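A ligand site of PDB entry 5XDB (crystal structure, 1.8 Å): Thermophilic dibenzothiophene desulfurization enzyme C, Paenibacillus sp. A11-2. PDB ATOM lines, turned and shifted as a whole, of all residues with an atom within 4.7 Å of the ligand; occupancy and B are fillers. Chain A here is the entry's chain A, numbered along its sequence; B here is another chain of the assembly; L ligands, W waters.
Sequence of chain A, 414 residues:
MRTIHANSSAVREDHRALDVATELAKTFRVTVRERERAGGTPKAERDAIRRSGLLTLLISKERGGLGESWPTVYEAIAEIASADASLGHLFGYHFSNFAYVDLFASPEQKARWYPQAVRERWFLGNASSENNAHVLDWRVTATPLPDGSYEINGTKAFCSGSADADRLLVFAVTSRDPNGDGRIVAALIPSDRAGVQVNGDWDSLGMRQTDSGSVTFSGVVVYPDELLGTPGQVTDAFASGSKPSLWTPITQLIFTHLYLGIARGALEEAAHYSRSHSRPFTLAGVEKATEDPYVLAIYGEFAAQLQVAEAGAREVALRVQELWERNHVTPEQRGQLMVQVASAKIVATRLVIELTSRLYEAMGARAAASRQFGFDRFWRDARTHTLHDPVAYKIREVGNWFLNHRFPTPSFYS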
ATOM      1  N   HIS A  89       1.415 -17.521 -30.354  1.00  0.00           N
ATOM      2  CA  HIS A  89       1.941 -17.267 -29.019  1.00  0.00           C
ATOM      3  C   HIS A  89       2.720 -18.474 -28.504  1.00  0.00           C
ATOM      4  O   HIS A  89       3.824 -18.324 -27.979  1.00  0.00           O
ATOM      5  CB  HIS A  89       0.772 -16.933 -28.081  1.00  0.00           C
ATOM      6  CG  HIS A  89       1.150 -16.879 -26.639  1.00  0.00           C
ATOM      7  ND1 HIS A  89       1.437 -15.697 -25.990  1.00  0.00           N
ATOM      8  CD2 HIS A  89       1.249 -17.852 -25.703  1.00  0.00           C
ATOM      9  CE1 HIS A  89       1.706 -15.952 -24.713  1.00  0.00           C
ATOM     10  NE2 HIS A  89       1.611 -17.253 -24.517  1.00  0.00           N
ATOM     11  N   TYR A  93       6.541 -18.211 -27.734  1.00  0.00           N
ATOM     12  CA  TYR A  93       7.077 -18.411 -26.394  1.00  0.00           C
ATOM     13  C   TYR A  93       8.036 -19.591 -26.346  1.00  0.00           C
ATOM     14  O   TYR A  93       8.976 -19.582 -25.542  1.00  0.00           O
ATOM     15  CB  TYR A  93       5.943 -18.599 -25.376  1.00  0.00           C
ATOM     16  CG  TYR A  93       5.975 -17.546 -24.282  1.00  0.00           C
ATOM     17  CD1 TYR A  93       7.067 -17.441 -23.418  1.00  0.00           C
ATOM     18  CD2 TYR A  93       4.921 -16.667 -24.114  1.00  0.00           C
ATOM     19  CE1 TYR A  93       7.104 -16.460 -22.410  1.00  0.00           C
ATOM     20  CE2 TYR A  93       4.938 -15.688 -23.121  1.00  0.00           C
ATOM     21  CZ  TYR A  93       6.033 -15.580 -22.274  1.00  0.00           C
ATOM     22  OH  TYR A  93       6.039 -14.614 -21.280  1.00  0.00           O
ATOM     23  N   ASN A 126       6.771 -22.750 -20.077  1.00  0.00           N
ATOM     24  CA  ASN A 126       7.478 -22.112 -18.973  1.00  0.00           C
ATOM     25  C   ASN A 126       6.545 -21.880 -17.802  1.00  0.00           C
ATOM     26  O   ASN A 126       5.318 -21.789 -17.950  1.00  0.00           O
ATOM     27  CB  ASN A 126       8.115 -20.768 -19.395  1.00  0.00           C
ATOM     28  CG  ASN A 126       7.112 -19.640 -19.475  1.00  0.00           C
ATOM     29  OD1 ASN A 126       6.994 -18.824 -18.546  1.00  0.00           O
ATOM     30  ND2 ASN A 126       6.373 -19.596 -20.585  1.00  0.00           N
ATOM     31  N   SER A 128       7.032 -19.180 -14.773  1.00  0.00           N
ATOM     32  CA  SER A 128       7.918 -18.106 -14.330  1.00  0.00           C
ATOM     33  C   SER A 128       7.192 -17.083 -13.451  1.00  0.00           C
ATOM     34  O   SER A 128       7.603 -16.834 -12.303  1.00  0.00           O
ATOM     35  CB  SER A 128       8.519 -17.398 -15.544  1.00  0.00           C
ATOM     36  OG  SER A 128       8.906 -18.322 -16.554  1.00  0.00           O
ATOM     37  N   SER A 129       6.130 -16.482 -13.978  1.00  0.00           N
ATOM     38  CA  SER A 129       5.386 -15.470 -13.257  1.00  0.00           C
ATOM     39  C   SER A 129       4.526 -16.082 -12.152  1.00  0.00           C
ATOM     40  O   SER A 129       4.268 -17.292 -12.117  1.00  0.00           O
ATOM     41  CB  SER A 129       4.503 -14.668 -14.211  1.00  0.00           C
ATOM     42  OG  SER A 129       5.279 -13.969 -15.166  1.00  0.00           O
ATOM     43  N   VAL A 135       4.138  -7.996  -9.408  1.00  0.00           N
ATOM     44  CA  VAL A 135       4.919  -8.853 -10.288  1.00  0.00           C
ATOM     45  C   VAL A 135       6.293  -9.198  -9.718  1.00  0.00           C
ATOM     46  O   VAL A 135       6.921 -10.171 -10.154  1.00  0.00           O
ATOM     47  CB  VAL A 135       5.090  -8.211 -11.678  1.00  0.00           C
ATOM     48  CG1 VAL A 135       3.792  -8.331 -12.479  1.00  0.00           C
ATOM     49  CG2 VAL A 135       5.515  -6.754 -11.538  1.00  0.00           C
ATOM     50  N   PHE A 158       0.189 -17.845 -15.130  1.00  0.00           N
ATOM     51  CA  PHE A 158       0.420 -17.507 -16.542  1.00  0.00           C
ATOM     52  C   PHE A 158       1.507 -18.382 -17.153  1.00  0.00           C
ATOM     53  O   PHE A 158       2.473 -17.894 -17.756  1.00  0.00           O
ATOM     54  CB  PHE A 158       0.778 -16.022 -16.696  1.00  0.00           C
ATOM     55  CG  PHE A 158      -0.392 -15.083 -16.517  1.00  0.00           C
ATOM     56  CD1 PHE A 158      -1.305 -14.895 -17.545  1.00  0.00           C
ATOM     57  CD2 PHE A 158      -0.543 -14.372 -15.343  1.00  0.00           C
ATOM     58  CE1 PHE A 158      -2.381 -14.009 -17.397  1.00  0.00           C
ATOM     59  CE2 PHE A 158      -1.612 -13.489 -15.183  1.00  0.00           C
ATOM     60  CZ  PHE A 158      -2.530 -13.306 -16.218  1.00  0.00           C
ATOM     61  N   CYS A 159       1.337 -19.695 -17.028  1.00  0.00           N
ATOM     62  CA  CYS A 159       2.352 -20.656 -17.468  1.00  0.00           C
ATOM     63  C   CYS A 159       2.078 -21.084 -18.909  1.00  0.00           C
ATOM     64  O   CYS A 159       1.603 -22.181 -19.181  1.00  0.00           O
ATOM     65  CB  CYS A 159       2.390 -21.848 -16.516  1.00  0.00           C
ATOM     66  SG  CYS A 159       2.838 -21.441 -14.837  1.00  0.00           S
ATOM     67  N   SER A 160       2.396 -20.184 -19.847  1.00  0.00           N
ATOM     68  CA  SER A 160       2.041 -20.431 -21.246  1.00  0.00           C
ATOM     69  C   SER A 160       2.674 -21.721 -21.745  1.00  0.00           C
ATOM     70  O   SER A 160       3.841 -22.006 -21.477  1.00  0.00           O
ATOM     71  CB  SER A 160       2.492 -19.270 -22.136  1.00  0.00           C
ATOM     72  OG  SER A 160       1.641 -18.145 -21.978  1.00  0.00           O
ATOM     73  N   TRP A 202      -6.994 -22.122 -17.365  1.00  0.00           N
ATOM     74  CA  TRP A 202      -6.955 -21.005 -18.295  1.00  0.00           C
ATOM     75  C   TRP A 202      -8.306 -20.867 -18.990  1.00  0.00           C
ATOM     76  O   TRP A 202      -8.740 -21.772 -19.709  1.00  0.00           O
ATOM     77  CB  TRP A 202      -5.846 -21.224 -19.334  1.00  0.00           C
ATOM     78  CG  TRP A 202      -5.635 -20.086 -20.284  1.00  0.00           C
ATOM     79  CD1 TRP A 202      -5.730 -20.142 -21.646  1.00  0.00           C
ATOM     80  CD2 TRP A 202      -5.245 -18.737 -19.965  1.00  0.00           C
ATOM     81  NE1 TRP A 202      -5.440 -18.917 -22.187  1.00  0.00           N
ATOM     82  CE2 TRP A 202      -5.137 -18.036 -21.183  1.00  0.00           C
ATOM     83  CE3 TRP A 202      -4.988 -18.065 -18.771  1.00  0.00           C
ATOM     84  CZ2 TRP A 202      -4.772 -16.686 -21.245  1.00  0.00           C
ATOM     85  CZ3 TRP A 202      -4.632 -16.714 -18.829  1.00  0.00           C
ATOM     86  CH2 TRP A 202      -4.533 -16.046 -20.059  1.00  0.00           C
ATOM     87  N   MET A 207      -6.605 -15.259 -26.609  1.00  0.00           N
ATOM     88  CA  MET A 207      -5.458 -16.157 -26.437  1.00  0.00           C
ATOM     89  C   MET A 207      -5.919 -17.441 -25.739  1.00  0.00           C
ATOM     90  O   MET A 207      -5.264 -17.965 -24.837  1.00  0.00           O
ATOM     91  CB  MET A 207      -4.323 -15.457 -25.683  1.00  0.00           C
ATOM     92  CG  MET A 207      -3.694 -14.302 -26.496  1.00  0.00           C
ATOM     93  SD  MET A 207      -2.850 -14.954 -27.955  1.00  0.00           S
ATOM     94  CE  MET A 207      -1.998 -13.517 -28.597  1.00  0.00           C
ATOM     95  N   SER A 212      -2.282 -20.838 -20.557  1.00  0.00           N
ATOM     96  CA  SER A 212      -1.509 -19.966 -19.672  1.00  0.00           C
ATOM     97  C   SER A 212      -2.061 -19.948 -18.258  1.00  0.00           C
ATOM     98  O   SER A 212      -2.130 -18.897 -17.620  1.00  0.00           O
ATOM     99  CB  SER A 212      -1.469 -18.556 -20.254  1.00  0.00           C
ATOM    100  OG  SER A 212      -0.888 -18.593 -21.549  1.00  0.00           O
ATOM    101  N   THR A 384      -6.135  -9.114 -25.093  1.00  0.00           N
ATOM    102  CA  THR A 384      -5.618  -9.903 -23.975  1.00  0.00           C
ATOM    103  C   THR A 384      -4.101  -9.812 -23.922  1.00  0.00           C
ATOM    104  O   THR A 384      -3.523  -9.507 -22.872  1.00  0.00           O
ATOM    105  CB  THR A 384      -6.045 -11.373 -24.117  1.00  0.00           C
ATOM    106  OG1 THR A 384      -7.474 -11.459 -24.116  1.00  0.00           O
ATOM    107  CG2 THR A 384      -5.500 -12.217 -22.962  1.00  0.00           C
ATOM    108  N   HIS A 385      -3.437 -10.069 -25.040  1.00  0.00           N
ATOM    109  CA  HIS A 385      -1.989 -10.226 -24.961  1.00  0.00           C
ATOM    110  C   HIS A 385      -1.280  -8.891 -24.724  1.00  0.00           C
ATOM    111  O   HIS A 385      -0.271  -8.855 -24.007  1.00  0.00           O
ATOM    112  CB  HIS A 385      -1.445 -10.884 -26.213  1.00  0.00           C
ATOM    113  CG  HIS A 385      -0.092 -11.478 -26.010  1.00  0.00           C
ATOM    114  ND1 HIS A 385       1.025 -10.704 -25.802  1.00  0.00           N
ATOM    115  CD2 HIS A 385       0.311 -12.765 -25.926  1.00  0.00           C
ATOM    116  CE1 HIS A 385       2.073 -11.487 -25.613  1.00  0.00           C
ATOM    117  NE2 HIS A 385       1.662 -12.739 -25.689  1.00  0.00           N
ATOM    118  N   LEU A 387      -1.729  -6.706 -22.793  1.00  0.00           N
ATOM    119  CA  LEU A 387      -1.671  -6.385 -21.382  1.00  0.00           C
ATOM    120  C   LEU A 387      -0.577  -7.177 -20.668  1.00  0.00           C
ATOM    121  O   LEU A 387      -0.433  -7.029 -19.455  1.00  0.00           O
ATOM    122  CB  LEU A 387      -3.031  -6.660 -20.728  1.00  0.00           C
ATOM    123  CG  LEU A 387      -4.229  -5.926 -21.353  1.00  0.00           C
ATOM    124  CD1 LEU A 387      -5.550  -6.521 -20.846  1.00  0.00           C
ATOM    125  CD2 LEU A 387      -4.143  -4.401 -21.048  1.00  0.00           C
ATOM    126  N   HIS A 388       0.163  -8.005 -21.396  1.00  0.00           N
ATOM    127  CA  HIS A 388       1.211  -8.833 -20.806  1.00  0.00           C
ATOM    128  C   HIS A 388       2.116  -8.011 -19.882  1.00  0.00           C
ATOM    129  O   HIS A 388       2.376  -8.401 -18.735  1.00  0.00           O
ATOM    130  CB  HIS A 388       2.027  -9.494 -21.916  1.00  0.00           C
ATOM    131  CG  HIS A 388       3.097 -10.417 -21.422  1.00  0.00           C
ATOM    132  ND1 HIS A 388       4.289  -9.972 -20.914  1.00  0.00           N
ATOM    133  CD2 HIS A 388       3.153 -11.779 -21.380  1.00  0.00           C
ATOM    134  CE1 HIS A 388       5.037 -11.007 -20.559  1.00  0.00           C
ATOM    135  NE2 HIS A 388       4.374 -12.109 -20.840  1.00  0.00           N
ATOM    136  N   TYR A 413      11.560  -7.745 -17.770  1.00  0.00           N
ATOM    137  CA  TYR A 413      10.566  -6.964 -18.507  1.00  0.00           C
ATOM    138  C   TYR A 413      11.167  -5.833 -19.327  1.00  0.00           C
ATOM    139  O   TYR A 413      10.466  -5.287 -20.192  1.00  0.00           O
ATOM    140  CB  TYR A 413       9.503  -6.404 -17.548  1.00  0.00           C
ATOM    141  CG  TYR A 413       8.940  -7.411 -16.566  1.00  0.00           C
ATOM    142  CD1 TYR A 413       7.708  -8.025 -16.794  1.00  0.00           C
ATOM    143  CD2 TYR A 413       9.650  -7.756 -15.414  1.00  0.00           C
ATOM    144  CE1 TYR A 413       7.199  -8.946 -15.891  1.00  0.00           C
ATOM    145  CE2 TYR A 413       9.140  -8.678 -14.512  1.00  0.00           C
ATOM    146  CZ  TYR A 413       7.915  -9.261 -14.751  1.00  0.00           C
ATOM    147  OH  TYR A 413       7.419 -10.178 -13.846  1.00  0.00           O
ATOM    148  N   ARG B 279      -3.336  -4.641  -9.679  1.00  0.00           N
ATOM    149  CA  ARG B 279      -2.121  -4.666  -8.890  1.00  0.00           C
ATOM    150  C   ARG B 279      -1.190  -3.532  -9.293  1.00  0.00           C
ATOM    151  O   ARG B 279      -1.083  -3.220 -10.491  1.00  0.00           O
ATOM    152  CB  ARG B 279      -1.391  -6.002  -9.058  1.00  0.00           C
ATOM    153  CG  ARG B 279      -2.074  -7.156  -8.323  1.00  0.00           C
ATOM    154  CD  ARG B 279      -2.145  -8.422  -9.175  1.00  0.00           C
ATOM    155  NE  ARG B 279      -0.958  -9.261  -9.040  1.00  0.00           N
ATOM    156  CZ  ARG B 279      -0.282  -9.770 -10.068  1.00  0.00           C
ATOM    157  NH1 ARG B 279      -0.677  -9.543 -11.319  1.00  0.00           N
ATOM    158  NH2 ARG B 279       0.781 -10.535  -9.832  1.00  0.00           N
ATOM    159  N   GLY B 364      -5.468  -3.958 -16.243  1.00  0.00           N
ATOM    160  CA  GLY B 364      -4.401  -4.931 -16.188  1.00  0.00           C
ATOM    161  C   GLY B 364      -4.786  -6.265 -16.834  1.00  0.00           C
ATOM    162  O   GLY B 364      -5.931  -6.519 -17.192  1.00  0.00           O
ATOM    163  N   ALA B 365      -3.781  -7.124 -16.946  1.00  0.00           N
ATOM    164  CA  ALA B 365      -3.935  -8.358 -17.703  1.00  0.00           C
ATOM    165  C   ALA B 365      -5.040  -9.235 -17.124  1.00  0.00           C
ATOM    166  O   ALA B 365      -5.794  -9.872 -17.873  1.00  0.00           O
ATOM    167  CB  ALA B 365      -2.620  -9.132 -17.759  1.00  0.00           C
ATOM    168  N   ARG B 366      -5.176  -9.281 -15.798  1.00  0.00           N
ATOM    169  CA  ARG B 366      -6.128 -10.206 -15.205  1.00  0.00           C
ATOM    170  C   ARG B 366      -7.571  -9.856 -15.548  1.00  0.00           C
ATOM    171  O   ARG B 366      -8.439 -10.727 -15.478  1.00  0.00           O
ATOM    172  CB  ARG B 366      -5.930 -10.269 -13.683  1.00  0.00           C
ATOM    173  CG  ARG B 366      -4.656 -11.012 -13.273  1.00  0.00           C
ATOM    174  CD  ARG B 366      -3.876 -10.275 -12.173  1.00  0.00           C
ATOM    175  NE  ARG B 366      -4.614 -10.273 -10.911  1.00  0.00           N
ATOM    176  CZ  ARG B 366      -5.086  -9.177 -10.328  1.00  0.00           C
ATOM    177  NH1 ARG B 366      -4.909  -7.990 -10.885  1.00  0.00           N
ATOM    178  NH2 ARG B 366      -5.754  -9.267  -9.177  1.00  0.00           N
HETATM  179  N1  LIG L   1       4.236 -14.589 -17.788  1.00  0.00           N
HETATM  180  C1  LIG L   1       5.255 -15.508 -17.784  1.00  0.00           C
HETATM  181  O1  LIG L   1       6.132 -15.420 -16.917  1.00  0.00           O
HETATM  182  N2  LIG L   1       5.273 -16.523 -18.730  1.00  0.00           N
HETATM  183  C2  LIG L   1       4.273 -16.606 -19.678  1.00  0.00           C
HETATM  184  O2  LIG L   1       4.287 -17.524 -20.515  1.00  0.00           O
HETATM  185  C3  LIG L   1       3.240 -15.658 -19.668  1.00  0.00           C
HETATM  186  N3  LIG L   1       2.227 -15.733 -20.599  1.00  0.00           N
HETATM  187  C4  LIG L   1       1.214 -14.795 -20.593  1.00  0.00           C
HETATM  188  C5  LIG L   1       0.212 -14.880 -21.565  1.00  0.00           C
HETATM  189  C6  LIG L   1      -0.825 -13.948 -21.582  1.00  0.00           C
HETATM  190  C7  LIG L   1      -1.888 -14.095 -22.637  1.00  0.00           C
HETATM  191  C8  LIG L   1      -0.847 -12.927 -20.623  1.00  0.00           C
HETATM  192  C9  LIG L   1      -1.937 -11.903 -20.579  1.00  0.00           C
HETATM  193  C10 LIG L   1       0.159 -12.848 -19.663  1.00  0.00           C
HETATM  194  C11 LIG L   1       1.201 -13.774 -19.639  1.00  0.00           C
HETATM  195  N4  LIG L   1       2.225 -13.685 -18.711  1.00  0.00           N
HETATM  196  C12 LIG L   1       3.225 -14.651 -18.717  1.00  0.00           C
HETATM  197  C13 LIG L   1       2.190 -12.678 -17.585  1.00  0.00           C
HETATM  198  C14 LIG L   1       2.637 -11.230 -17.656  1.00  0.00           C
HETATM  199  O3  LIG L   1       4.049 -11.220 -17.702  1.00  0.00           O
HETATM  200  C15 LIG L   1       2.177 -10.536 -16.356  1.00  0.00           C
HETATM  201  O4  LIG L   1       2.569 -11.332 -15.256  1.00  0.00           O
HETATM  202  C16 LIG L   1       0.670 -10.293 -16.218  1.00  0.00           C
HETATM  203  O5  LIG L   1       0.180  -9.794 -17.444  1.00  0.00           O
HETATM  204  C17 LIG L   1       0.367  -9.311 -15.080  1.00  0.00           C
HETATM  205  O6  LIG L   1      -1.026  -9.262 -14.774  1.00  0.00           O
HETATM  206  P1  LIG L   1      -1.737  -7.901 -14.240  1.00  0.00           P
HETATM  207  O7  LIG L   1      -1.545  -6.831 -15.321  1.00  0.00           O
HETATM  208  O8  LIG L   1      -3.223  -8.121 -14.014  1.00  0.00           O
HETATM  209  O9  LIG L   1      -1.135  -7.466 -12.930  1.00  0.00           O
HETATM  210  O   HOH W   1      -5.614  -6.793 -13.669  1.00  0.00           O
HETATM  211  O   HOH W   2       4.615 -18.135 -15.994  1.00  0.00           O
HETATM  212  O   HOH W   3       1.385 -12.396 -13.065  1.00  0.00           O
HETATM  213  O   HOH W   4      -3.102  -5.691 -12.254  1.00  0.00           O
HETATM  214  O   HOH W   5       0.854  -6.004 -12.744  1.00  0.00           O
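The backbone carbonyl oxygen (O) of Leu 387 is in hydrogen-bond range of an oxygen (O5) of the ligand, at 3.5 Å.
An oxygen (O8) of the ligand is in salt-bridge range of the guanidinium group (NH1) of Arg 366 of chain B, at 3.6 Å.
N of Arg 366 of chain B lies within hydrogen-bond range of O8 of the ligand (2.9 Å).
The side-chain hydroxyl of Ser 160 lies within hydrogen-bond range of a nitrogen (N3) of the ligand.
The backbone NH (N) of Ala 365 of chain B is in hydrogen-bond range of an oxygen (O7) of the ligand, at 2.8 Å.
A nitrogen (N2) of the ligand lies within hydrogen-bond range of the side-chain amide oxygen of Asn 126, 2.9 Å away.
The backbone NH of Ser 129 sits at hydrogen-bond distance from an oxygen (O1) of the ligand, at 3.1 Å.
The backbone carbonyl oxygen (O) of Phe 158 lies close to a nitrogen (N2) of the ligand (3.3 Å).
O3 of the ligand sits close to NE2 of His 388, 3.3 Å away.
N2 of the ligand lies close to OH of Tyr 93.
O9 of the ligand lies within salt-bridge range of NH1 of Arg 279 of chain B (2.7 Å).
OG of Ser 129 is in hydrogen-bond range of O1 of the ligand, 2.4 Å away.
An oxygen (O5) of the ligand lies within hydrogen-bond range of the backbone carbonyl oxygen of His 388 (2.9 Å).
The backbone NH (N) of Ser 160 lies close to an oxygen (O2) of the ligand (3.3 Å).
O of Ser 160 is in hydrogen-bond range of N of Asn 126, at 3.3 Å.
The side-chain hydroxyl (OG) of Ser 160 is in hydrogen-bond range of the side-chain hydroxyl (OG) of Ser 212, at 2.6 Å.
OG of Ser 128 is in hydrogen-bond range of OD1 of Asn 126 (2.8 Å).
A ring nitrogen (NE2) of His 388 sits at hydrogen-bond distance from the side-chain hydroxyl (OH) of Tyr 93, 3.0 Å away.
ND1 of His 89 sits at hydrogen-bond distance from NE2 of His 385 (3.0 Å).
OG of Ser 160 sits at hydrogen-bond distance from NE2 of His 89 (2.7 Å).
Residues that only touch the ligand: Ser 128 (3.4 Å), Gly 364 of chain B (3.5 Å), His 89 (3.6 Å), Thr 384 (3.7 Å) and Ser 212 (3.9 Å).
Hydrophobic or aromatic side chains that line the ligand: His 89, Tyr 93, Phe 158, His 388 and Ala 365 of chain B.
Within 4 Å of the ligand: His 89, Tyr 93, Asn 126, Ser 128, Ser 129, Phe 158, Ser 160, Ser 212, Thr 384, Leu 387, His 388, Arg 279 of chain B, Gly 364 of chain B, Ala 365 of chain B and Arg 366 of chain B.
The nearest printed residue that does not touch the ligand is Trp 202 (4.1 Å).
Water W4 lies within hydrogen-bond range of O9 of the ligand, N of Arg 279 of chain B and NH1 of Arg 366 of chain B.
Water W1 bridges O8 of the ligand and NH1 of Arg 366 of chain B.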
